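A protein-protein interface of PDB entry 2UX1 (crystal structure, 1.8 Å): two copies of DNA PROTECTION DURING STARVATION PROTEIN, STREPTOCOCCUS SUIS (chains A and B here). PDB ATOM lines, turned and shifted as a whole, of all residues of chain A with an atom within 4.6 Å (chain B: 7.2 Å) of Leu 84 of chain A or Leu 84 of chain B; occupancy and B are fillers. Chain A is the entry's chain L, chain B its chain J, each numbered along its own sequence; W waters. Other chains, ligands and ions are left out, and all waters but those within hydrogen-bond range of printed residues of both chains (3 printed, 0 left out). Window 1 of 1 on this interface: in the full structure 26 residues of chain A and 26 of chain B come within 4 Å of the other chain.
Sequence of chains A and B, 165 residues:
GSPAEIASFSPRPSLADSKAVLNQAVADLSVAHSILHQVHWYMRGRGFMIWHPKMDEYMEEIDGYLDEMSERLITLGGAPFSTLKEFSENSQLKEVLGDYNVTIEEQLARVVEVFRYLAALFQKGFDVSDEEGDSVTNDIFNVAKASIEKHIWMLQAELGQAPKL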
ATOM      1  N   VAL A  31     -32.661  11.632 -32.913  1.00  0.00           N
ATOM      2  CA  VAL A  31     -32.558  12.445 -31.700  1.00  0.00           C
ATOM      3  C   VAL A  31     -33.930  12.580 -31.030  1.00  0.00           C
ATOM      4  O   VAL A  31     -34.035  12.503 -29.798  1.00  0.00           O
ATOM      5  CB  VAL A  31     -31.850  13.811 -31.974  1.00  0.00           C
ATOM      6  CG1 VAL A  31     -31.890  14.729 -30.744  1.00  0.00           C
ATOM      7  CG2 VAL A  31     -30.394  13.566 -32.376  1.00  0.00           C
ATOM      8  N   SER A  34     -34.681   9.610 -28.970  1.00  0.00           N
ATOM      9  CA  SER A  34     -33.910   9.697 -27.733  1.00  0.00           C
ATOM     10  C   SER A  34     -34.604  10.608 -26.708  1.00  0.00           C
ATOM     11  O   SER A  34     -34.731  10.258 -25.550  1.00  0.00           O
ATOM     12  CB  SER A  34     -32.508  10.224 -28.046  1.00  0.00           C
ATOM     13  OG  SER A  34     -31.682  10.165 -26.904  1.00  0.00           O
ATOM     14  N   THR A  83     -24.875   6.416 -37.635  1.00  0.00           N
ATOM     15  CA  THR A  83     -24.056   6.347 -36.402  1.00  0.00           C
ATOM     16  C   THR A  83     -24.541   7.435 -35.444  1.00  0.00           C
ATOM     17  O   THR A  83     -25.105   8.433 -35.878  1.00  0.00           O
ATOM     18  CB  THR A  83     -22.551   6.563 -36.674  1.00  0.00           C
ATOM     19  OG1 THR A  83     -22.363   7.797 -37.368  1.00  0.00           O
ATOM     20  CG2 THR A  83     -21.961   5.442 -37.494  1.00  0.00           C
ATOM     21  N   LEU A  84     -24.353   7.221 -34.144  1.00  0.00           N
ATOM     22  CA  LEU A  84     -24.789   8.191 -33.152  1.00  0.00           C
ATOM     23  C   LEU A  84     -24.059   9.511 -33.340  1.00  0.00           C
ATOM     24  O   LEU A  84     -24.671  10.575 -33.221  1.00  0.00           O
ATOM     25  CB  LEU A  84     -24.599   7.644 -31.724  1.00  0.00           C
ATOM     26  CG  LEU A  84     -25.456   6.449 -31.287  1.00  0.00           C
ATOM     27  CD1 LEU A  84     -25.381   6.270 -29.779  1.00  0.00           C
ATOM     28  CD2 LEU A  84     -26.921   6.562 -31.740  1.00  0.00           C
ATOM     29  N   LYS A  85     -22.776   9.451 -33.701  1.00  0.00           N
ATOM     30  CA  LYS A  85     -22.026  10.688 -33.976  1.00  0.00           C
ATOM     31  C   LYS A  85     -22.705  11.490 -35.091  1.00  0.00           C
ATOM     32  O   LYS A  85     -22.973  12.678 -34.932  1.00  0.00           O
ATOM     33  CB  LYS A  85     -20.570  10.386 -34.320  1.00  0.00           C
ATOM     34  CG  LYS A  85     -19.729  11.629 -34.694  1.00  0.00           C
ATOM     35  CD  LYS A  85     -18.253  11.267 -34.827  1.00  0.00           C
ATOM     36  CE  LYS A  85     -17.522  12.230 -35.759  1.00  0.00           C
ATOM     37  NZ  LYS A  85     -16.471  11.517 -36.558  1.00  0.00           N
ATOM     38  N   GLU A  86     -23.010  10.824 -36.202  1.00  0.00           N
ATOM     39  CA  GLU A  86     -23.675  11.467 -37.335  1.00  0.00           C
ATOM     40  C   GLU A  86     -25.032  12.041 -36.966  1.00  0.00           C
ATOM     41  O   GLU A  86     -25.359  13.151 -37.375  1.00  0.00           O
ATOM     42  CB  GLU A  86     -23.871  10.476 -38.475  1.00  0.00           C
ATOM     43  CG  GLU A  86     -22.634  10.150 -39.274  1.00  0.00           C
ATOM     44  CD  GLU A  86     -22.915   9.114 -40.352  1.00  0.00           C
ATOM     45  OE1 GLU A  86     -23.154   7.945 -39.990  1.00  0.00           O
ATOM     46  OE2 GLU A  86     -22.890   9.458 -41.563  1.00  0.00           O
ATOM     47  N   PHE A  87     -25.841  11.276 -36.218  1.00  0.00           N
ATOM     48  CA  PHE A  87     -27.163  11.758 -35.794  1.00  0.00           C
ATOM     49  C   PHE A  87     -27.038  13.046 -34.988  1.00  0.00           C
ATOM     50  O   PHE A  87     -27.679  14.054 -35.288  1.00  0.00           O
ATOM     51  CB  PHE A  87     -27.932  10.713 -34.961  1.00  0.00           C
ATOM     52  CG  PHE A  87     -28.208   9.419 -35.688  1.00  0.00           C
ATOM     53  CD1 PHE A  87     -28.527   9.406 -37.047  1.00  0.00           C
ATOM     54  CD2 PHE A  87     -28.170   8.201 -34.993  1.00  0.00           C
ATOM     55  CE1 PHE A  87     -28.777   8.189 -37.708  1.00  0.00           C
ATOM     56  CE2 PHE A  87     -28.425   7.007 -35.636  1.00  0.00           C
ATOM     57  CZ  PHE A  87     -28.727   6.999 -37.001  1.00  0.00           C
ATOM     58  N   SER A  88     -26.192  12.996 -33.967  1.00  0.00           N
ATOM     59  CA  SER A  88     -26.031  14.098 -33.028  1.00  0.00           C
ATOM     60  C   SER A  88     -25.487  15.349 -33.703  1.00  0.00           C
ATOM     61  O   SER A  88     -25.914  16.460 -33.392  1.00  0.00           O
ATOM     62  CB  SER A  88     -25.113  13.663 -31.884  1.00  0.00           C
ATOM     63  OG  SER A  88     -25.388  14.409 -30.717  1.00  0.00           O
ATOM     64  N   GLU A  95     -30.183  17.879 -26.978  1.00  0.00           N
ATOM     65  CA  GLU A  95     -30.483  17.000 -25.851  1.00  0.00           C
ATOM     66  C   GLU A  95     -29.885  17.523 -24.561  1.00  0.00           C
ATOM     67  O   GLU A  95     -28.771  18.035 -24.569  1.00  0.00           O
ATOM     68  CB  GLU A  95     -29.908  15.610 -26.113  1.00  0.00           C
ATOM     69  CG  GLU A  95     -30.505  14.901 -27.314  1.00  0.00           C
ATOM     70  CD  GLU A  95     -30.078  13.453 -27.367  1.00  0.00           C
ATOM     71  OE1 GLU A  95     -28.952  13.179 -27.838  1.00  0.00           O
ATOM     72  OE2 GLU A  95     -30.873  12.584 -26.935  1.00  0.00           O
ATOM     73  N   ALA B  27     -26.072   2.171 -22.434  1.00  0.00           N
ATOM     74  CA  ALA B  27     -25.235   2.798 -23.456  1.00  0.00           C
ATOM     75  C   ALA B  27     -24.886   1.820 -24.578  1.00  0.00           C
ATOM     76  O   ALA B  27     -25.054   2.123 -25.758  1.00  0.00           O
ATOM     77  CB  ALA B  27     -23.958   3.372 -22.817  1.00  0.00           C
ATOM     78  N   SER B  30     -27.777   0.755 -26.754  1.00  0.00           N
ATOM     79  CA  SER B  30     -28.130   1.861 -27.667  1.00  0.00           C
ATOM     80  C   SER B  30     -27.215   1.914 -28.881  1.00  0.00           C
ATOM     81  O   SER B  30     -27.651   2.243 -30.007  1.00  0.00           O
ATOM     82  CB  SER B  30     -28.072   3.222 -26.955  1.00  0.00           C
ATOM     83  OG  SER B  30     -28.988   3.297 -25.880  1.00  0.00           O
ATOM     84  N   VAL B  31     -25.934   1.667 -28.651  1.00  0.00           N
ATOM     85  CA  VAL B  31     -24.972   1.647 -29.747  1.00  0.00           C
ATOM     86  C   VAL B  31     -25.159   0.355 -30.539  1.00  0.00           C
ATOM     87  O   VAL B  31     -25.122   0.375 -31.775  1.00  0.00           O
ATOM     88  CB  VAL B  31     -23.516   1.877 -29.262  1.00  0.00           C
ATOM     89  CG1 VAL B  31     -22.524   1.677 -30.390  1.00  0.00           C
ATOM     90  CG2 VAL B  31     -23.382   3.281 -28.705  1.00  0.00           C
ATOM     91  N   ALA B  32     -25.391  -0.762 -29.840  1.00  0.00           N
ATOM     92  CA  ALA B  32     -25.687  -2.023 -30.544  1.00  0.00           C
ATOM     93  C   ALA B  32     -26.892  -1.861 -31.471  1.00  0.00           C
ATOM     94  O   ALA B  32     -26.840  -2.258 -32.641  1.00  0.00           O
ATOM     95  CB  ALA B  32     -25.894  -3.155 -29.589  1.00  0.00           C
ATOM     96  N   HIS B  33     -27.964  -1.247 -30.968  1.00  0.00           N
ATOM     97  CA  HIS B  33     -29.114  -0.953 -31.829  1.00  0.00           C
ATOM     98  C   HIS B  33     -28.702  -0.206 -33.100  1.00  0.00           C
ATOM     99  O   HIS B  33     -29.099  -0.578 -34.213  1.00  0.00           O
ATOM    100  CB  HIS B  33     -30.202  -0.148 -31.104  1.00  0.00           C
ATOM    101  CG  HIS B  33     -31.335   0.231 -32.008  1.00  0.00           C
ATOM    102  ND1 HIS B  33     -32.544  -0.430 -32.006  1.00  0.00           N
ATOM    103  CD2 HIS B  33     -31.419   1.167 -32.983  1.00  0.00           C
ATOM    104  CE1 HIS B  33     -33.333   0.103 -32.922  1.00  0.00           C
ATOM    105  NE2 HIS B  33     -32.667   1.060 -33.542  1.00  0.00           N
ATOM    106  N   SER B  34     -27.916   0.851 -32.924  1.00  0.00           N
ATOM    107  CA  SER B  34     -27.495   1.694 -34.034  1.00  0.00           C
ATOM    108  C   SER B  34     -26.666   0.911 -35.066  1.00  0.00           C
ATOM    109  O   SER B  34     -26.830   1.097 -36.266  1.00  0.00           O
ATOM    110  CB  SER B  34     -26.745   2.915 -33.489  1.00  0.00           C
ATOM    111  OG  SER B  34     -26.259   3.727 -34.530  1.00  0.00           O
ATOM    112  N   PHE B  81     -28.517   6.811 -18.467  1.00  0.00           N
ATOM    113  CA  PHE B  81     -28.061   7.608 -19.609  1.00  0.00           C
ATOM    114  C   PHE B  81     -29.252   7.735 -20.557  1.00  0.00           C
ATOM    115  O   PHE B  81     -30.006   6.779 -20.748  1.00  0.00           O
ATOM    116  CB  PHE B  81     -26.895   6.932 -20.333  1.00  0.00           C
ATOM    117  CG  PHE B  81     -25.676   6.673 -19.458  1.00  0.00           C
ATOM    118  CD1 PHE B  81     -25.124   7.687 -18.676  1.00  0.00           C
ATOM    119  CD2 PHE B  81     -25.054   5.425 -19.466  1.00  0.00           C
ATOM    120  CE1 PHE B  81     -23.997   7.446 -17.871  1.00  0.00           C
ATOM    121  CE2 PHE B  81     -23.921   5.179 -18.678  1.00  0.00           C
ATOM    122  CZ  PHE B  81     -23.399   6.194 -17.877  1.00  0.00           C
ATOM    123  N   SER B  82     -29.453   8.910 -21.128  1.00  0.00           N
ATOM    124  CA  SER B  82     -30.648   9.104 -21.910  1.00  0.00           C
ATOM    125  C   SER B  82     -30.435  10.117 -22.994  1.00  0.00           C
ATOM    126  O   SER B  82     -31.389  10.769 -23.429  1.00  0.00           O
ATOM    127  CB  SER B  82     -31.822   9.508 -21.021  1.00  0.00           C
ATOM    128  OG  SER B  82     -31.592  10.755 -20.405  1.00  0.00           O
ATOM    129  N   THR B  83     -29.181  10.257 -23.416  1.00  0.00           N
ATOM    130  CA  THR B  83     -28.811  11.185 -24.498  1.00  0.00           C
ATOM    131  C   THR B  83     -27.809  10.498 -25.412  1.00  0.00           C
ATOM    132  O   THR B  83     -27.041   9.657 -24.961  1.00  0.00           O
ATOM    133  CB  THR B  83     -28.164  12.504 -23.958  1.00  0.00           C
ATOM    134  OG1 THR B  83     -26.955  12.189 -23.270  1.00  0.00           O
ATOM    135  CG2 THR B  83     -29.100  13.220 -22.993  1.00  0.00           C
ATOM    136  N   LEU B  84     -27.789  10.861 -26.690  1.00  0.00           N
ATOM    137  CA  LEU B  84     -26.866  10.205 -27.623  1.00  0.00           C
ATOM    138  C   LEU B  84     -25.405  10.393 -27.189  1.00  0.00           C
ATOM    139  O   LEU B  84     -24.595   9.467 -27.293  1.00  0.00           O
ATOM    140  CB  LEU B  84     -27.085  10.693 -29.062  1.00  0.00           C
ATOM    141  CG  LEU B  84     -28.416  10.391 -29.761  1.00  0.00           C
ATOM    142  CD1 LEU B  84     -28.209  10.567 -31.257  1.00  0.00           C
ATOM    143  CD2 LEU B  84     -28.974   8.998 -29.450  1.00  0.00           C
ATOM    144  N   LYS B  85     -25.090  11.582 -26.667  1.00  0.00           N
ATOM    145  CA  LYS B  85     -23.749  11.898 -26.141  1.00  0.00           C
ATOM    146  C   LYS B  85     -23.344  10.898 -25.056  1.00  0.00           C
ATOM    147  O   LYS B  85     -22.278  10.288 -25.142  1.00  0.00           O
ATOM    148  CB  LYS B  85     -23.718  13.334 -25.609  1.00  0.00           C
ATOM    149  CG  LYS B  85     -22.341  13.991 -25.525  1.00  0.00           C
ATOM    150  CD  LYS B  85     -22.454  15.329 -24.780  1.00  0.00           C
ATOM    151  CE  LYS B  85     -21.308  16.294 -25.076  1.00  0.00           C
ATOM    152  NZ  LYS B  85     -19.952  15.728 -24.808  1.00  0.00           N
ATOM    153  N   GLU B  86     -24.203  10.705 -24.058  1.00  0.00           N
ATOM    154  CA  GLU B  86     -23.946   9.733 -22.986  1.00  0.00           C
ATOM    155  C   GLU B  86     -23.805   8.300 -23.479  1.00  0.00           C
ATOM    156  O   GLU B  86     -22.994   7.540 -22.954  1.00  0.00           O
ATOM    157  CB  GLU B  86     -25.060   9.770 -21.947  1.00  0.00           C
ATOM    158  CG  GLU B  86     -25.064  10.986 -21.052  1.00  0.00           C
ATOM    159  CD  GLU B  86     -26.278  11.030 -20.149  1.00  0.00           C
ATOM    160  OE1 GLU B  86     -27.391  11.316 -20.659  1.00  0.00           O
ATOM    161  OE2 GLU B  86     -26.125  10.793 -18.928  1.00  0.00           O
ATOM    162  N   PHE B  87     -24.618   7.915 -24.466  1.00  0.00           N
ATOM    163  CA  PHE B  87     -24.532   6.553 -25.007  1.00  0.00           C
ATOM    164  C   PHE B  87     -23.183   6.376 -25.682  1.00  0.00           C
ATOM    165  O   PHE B  87     -22.446   5.428 -25.392  1.00  0.00           O
ATOM    166  CB  PHE B  87     -25.654   6.252 -26.020  1.00  0.00           C
ATOM    167  CG  PHE B  87     -27.055   6.367 -25.457  1.00  0.00           C
ATOM    168  CD1 PHE B  87     -27.337   5.997 -24.144  1.00  0.00           C
ATOM    169  CD2 PHE B  87     -28.098   6.801 -26.268  1.00  0.00           C
ATOM    170  CE1 PHE B  87     -28.636   6.101 -23.634  1.00  0.00           C
ATOM    171  CE2 PHE B  87     -29.399   6.910 -25.776  1.00  0.00           C
ATOM    172  CZ  PHE B  87     -29.670   6.555 -24.452  1.00  0.00           C
ATOM    173  N   SER B  88     -22.877   7.324 -26.570  1.00  0.00           N
ATOM    174  CA  SER B  88     -21.678   7.303 -27.381  1.00  0.00           C
ATOM    175  C   SER B  88     -20.423   7.236 -26.512  1.00  0.00           C
ATOM    176  O   SER B  88     -19.558   6.377 -26.727  1.00  0.00           O
ATOM    177  CB  SER B  88     -21.651   8.545 -28.277  1.00  0.00           C
ATOM    178  OG  SER B  88     -21.066   8.243 -29.522  1.00  0.00           O
ATOM    179  N   GLU B  89     -20.363   8.114 -25.510  1.00  0.00           N
ATOM    180  CA  GLU B  89     -19.178   8.296 -24.668  1.00  0.00           C
ATOM    181  C   GLU B  89     -18.944   7.183 -23.660  1.00  0.00           C
ATOM    182  O   GLU B  89     -17.813   6.981 -23.220  1.00  0.00           O
ATOM    183  CB  GLU B  89     -19.253   9.634 -23.933  1.00  0.00           C
ATOM    184  CG  GLU B  89     -19.106  10.831 -24.864  1.00  0.00           C
ATOM    185  CD  GLU B  89     -19.125  12.177 -24.156  1.00  0.00           C
ATOM    186  OE1 GLU B  89     -19.174  12.230 -22.903  1.00  0.00           O
ATOM    187  OE2 GLU B  89     -19.091  13.201 -24.875  1.00  0.00           O
ATOM    188  N   ASN B  90     -20.011   6.477 -23.287  1.00  0.00           N
ATOM    189  CA  ASN B  90     -19.931   5.438 -22.268  1.00  0.00           C
ATOM    190  C   ASN B  90     -19.869   4.028 -22.832  1.00  0.00           C
ATOM    191  O   ASN B  90     -19.408   3.103 -22.164  1.00  0.00           O
ATOM    192  CB  ASN B  90     -21.092   5.564 -21.283  1.00  0.00           C
ATOM    193  CG  ASN B  90     -20.941   6.761 -20.361  1.00  0.00           C
ATOM    194  OD1 ASN B  90     -20.432   6.622 -19.247  1.00  0.00           O
ATOM    195  ND2 ASN B  90     -21.370   7.940 -20.817  1.00  0.00           N
ATOM    196  N   SER B  91     -20.326   3.860 -24.068  1.00  0.00           N
ATOM    197  CA  SER B  91     -20.299   2.551 -24.710  1.00  0.00           C
ATOM    198  C   SER B  91     -18.887   2.096 -25.050  1.00  0.00           C
ATOM    199  O   SER B  91     -18.045   2.900 -25.427  1.00  0.00           O
ATOM    200  CB  SER B  91     -21.141   2.564 -25.989  1.00  0.00           C
ATOM    201  OG  SER B  91     -21.224   1.261 -26.537  1.00  0.00           O
ATOM    202  N   GLU B  95     -18.482   2.547 -33.540  1.00  0.00           N
ATOM    203  CA  GLU B  95     -19.265   2.660 -34.763  1.00  0.00           C
ATOM    204  C   GLU B  95     -18.389   3.215 -35.873  1.00  0.00           C
ATOM    205  O   GLU B  95     -17.458   3.979 -35.606  1.00  0.00           O
ATOM    206  CB  GLU B  95     -20.427   3.623 -34.543  1.00  0.00           C
ATOM    207  CG  GLU B  95     -21.439   3.201 -33.475  1.00  0.00           C
ATOM    208  CD  GLU B  95     -22.669   4.117 -33.462  1.00  0.00           C
ATOM    209  OE1 GLU B  95     -22.588   5.227 -32.896  1.00  0.00           O
ATOM    210  OE2 GLU B  95     -23.716   3.727 -34.021  1.00  0.00           O
HETATM  211  O   HOH W   1     -21.017   7.238 -33.313  1.00  0.00           O
HETATM  212  O   HOH W   2     -32.561  13.008 -24.541  1.00  0.00           O
HETATM  213  O   HOH W   3     -26.876  14.111 -26.940  1.00  0.00           O
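The side-chain carboxylate of Glu 95 of chain B is in hydrogen-bond range of the backbone NH of Leu 84 of chain A (2.9 Å).
N of Leu 84 of chain B sits at hydrogen-bond distance from OE1 of Glu 95 of chain A, at 2.8 Å.
The side-chain hydroxyl (OG1) of Thr 83 of chain A sits at hydrogen-bond distance from the side-chain carboxylate (OE1) of Glu 86 of chain A (2.7 Å).
The side-chain carboxylate (OE2) of Glu 95 of chain A is in hydrogen-bond range of the side-chain hydroxyl (OG) of Ser 34 of chain A, at 2.6 Å.
The side-chain carboxylate (OE1) of Glu 86 of chain B sits at hydrogen-bond distance from the backbone NH (N) of Ser 82 of chain B (3.2 Å).
The side-chain hydroxyl of Ser 34 of chain B lies within hydrogen-bond range of the side-chain carboxylate of Glu 95 of chain B.
The side-chain hydroxyl of Thr 83 of chain B is in hydrogen-bond range of the side-chain carboxylate of Glu 86 of chain B (2.8 Å).
Among the printed residues, pairs that only touch across the chains: Glu 95 of chain A with Thr 83 of chain B (3.5 Å), Ser 34 of chain A with Ser 82 of chain B (3.5 Å), Thr 83 of chain A with Glu 95 of chain B (3.6 Å), Phe 87 of chain A with Leu 84 of chain B (3.7 Å), Leu 84 of chain A with Val 31 of chain B (3.8 Å), Leu 84 of chain A with Phe 87 of chain B (3.8 Å), Val 31 of chain A with Leu 84 of chain B (3.9 Å), Ser 34 of chain A with Thr 83 of chain B (3.9 Å), Ser 34 of chain A with Leu 84 of chain B (3.9 Å), Thr 83 of chain A with Ser 34 of chain B (3.9 Å), Leu 84 of chain A with Leu 84 of chain B (3.9 Å), Glu 95 of chain A with Ser 82 of chain B (3.98 Å) and Leu 84 of chain A with Ser 34 of chain B (3.999 Å).
Of the printed residues of chain B, Leu 84 of chain A touches Val 31 (3.8 Å), Ser 34 (3.999 Å), Leu 84 (3.9 Å), Phe 87 (3.8 Å) and Glu 95 (2.9 Å).
Of chain A, only Val 31 (3.9 Å), Ser 34 (3.9 Å), Leu 84 (3.9 Å), Phe 87 (3.7 Å) and Glu 95 (2.8 Å) come within 4 Å of Leu 84 of chain B.
Of the printed residues of chain A, Glu 95 of chain B touches Thr 83 (3.6 Å) and Leu 84 (2.9 Å).
Printed residues of chain B within 4 Å of Glu 95 of chain A: Ser 82, Thr 83 and Leu 84.
Of the printed residues of chain A, Val 31 of chain B touches Leu 84.
Printed residues of chain A within 4 Å of Ser 34 of chain B: Thr 83 and Leu 84.
Ala 27 of chain B touches none of the printed residues of chain A.
Glu 86 of chain B touches none of the printed residues of chain A.
The nearest printed residue of chain B that does not touch Leu 84 of chain A is Ser 88 of chain B (4.2 Å).
Printed residues of chain B that touch a printed residue of chain A: Val 31, Ser 34, Ser 82, Thr 83, Leu 84, Phe 87 and Glu 95.
Hydrophobic or aromatic side chains of chain B within 4 Å of the printed part of chain A: Val 31, Leu 84 and Phe 87.
Along chain B the printed residues that touch a printed residue of chain A span positions 31 to 95.
Of the 9 printed residues of chain A, 6 touch a printed residue of chain B.
Hydrophobic or aromatic side chains of chain A that line the printed part of chain B: Val 31, Leu 84 and Phe 87.
Among the printed residues, no Asp or Glu carboxylate lies within 4 Å of a Lys or Arg side-chain nitrogen of the other chain.
Val 31 of chain A touches Leu 84 of chain B, and with the chains exchanged Leu 84 of chain A touches Val 31 of chain B.
Ser 34 of chain A touches Thr 83 of chain B, and with the chains exchanged Thr 83 of chain A touches Ser 34 of chain B.
Leu 84 of chain A touches Phe 87 of chain B, and with the chains exchanged Phe 87 of chain A touches Leu 84 of chain B.
Leu 84 of chain A touches Glu 95 of chain B, and with the chains exchanged Glu 95 of chain A touches Leu 84 of chain B.
Positions printed for both chains: 31, 34, 83, 84, 85, 86, 87, 88 and 95.
Water W3 lies within hydrogen-bond range of OE1 of Glu 95 of chain A, N of Lys 85 of chain B and N of Leu 84 of chain B.
Water W1 lies within hydrogen-bond range of the side-chain carboxylate (OE1) of Glu 95 of chain B (2.6 Å), the backbone NH (N) of Lys 85 of chain A (2.9 Å) and the backbone NH (N) of Leu 84 of chain A (3.4 Å).
Water W2 lies within hydrogen-bond range of the backbone carbonyl oxygen of Ser 82 of chain B (2.8 Å) and the side-chain carboxylate of Glu 95 of chain A (3.0 Å).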
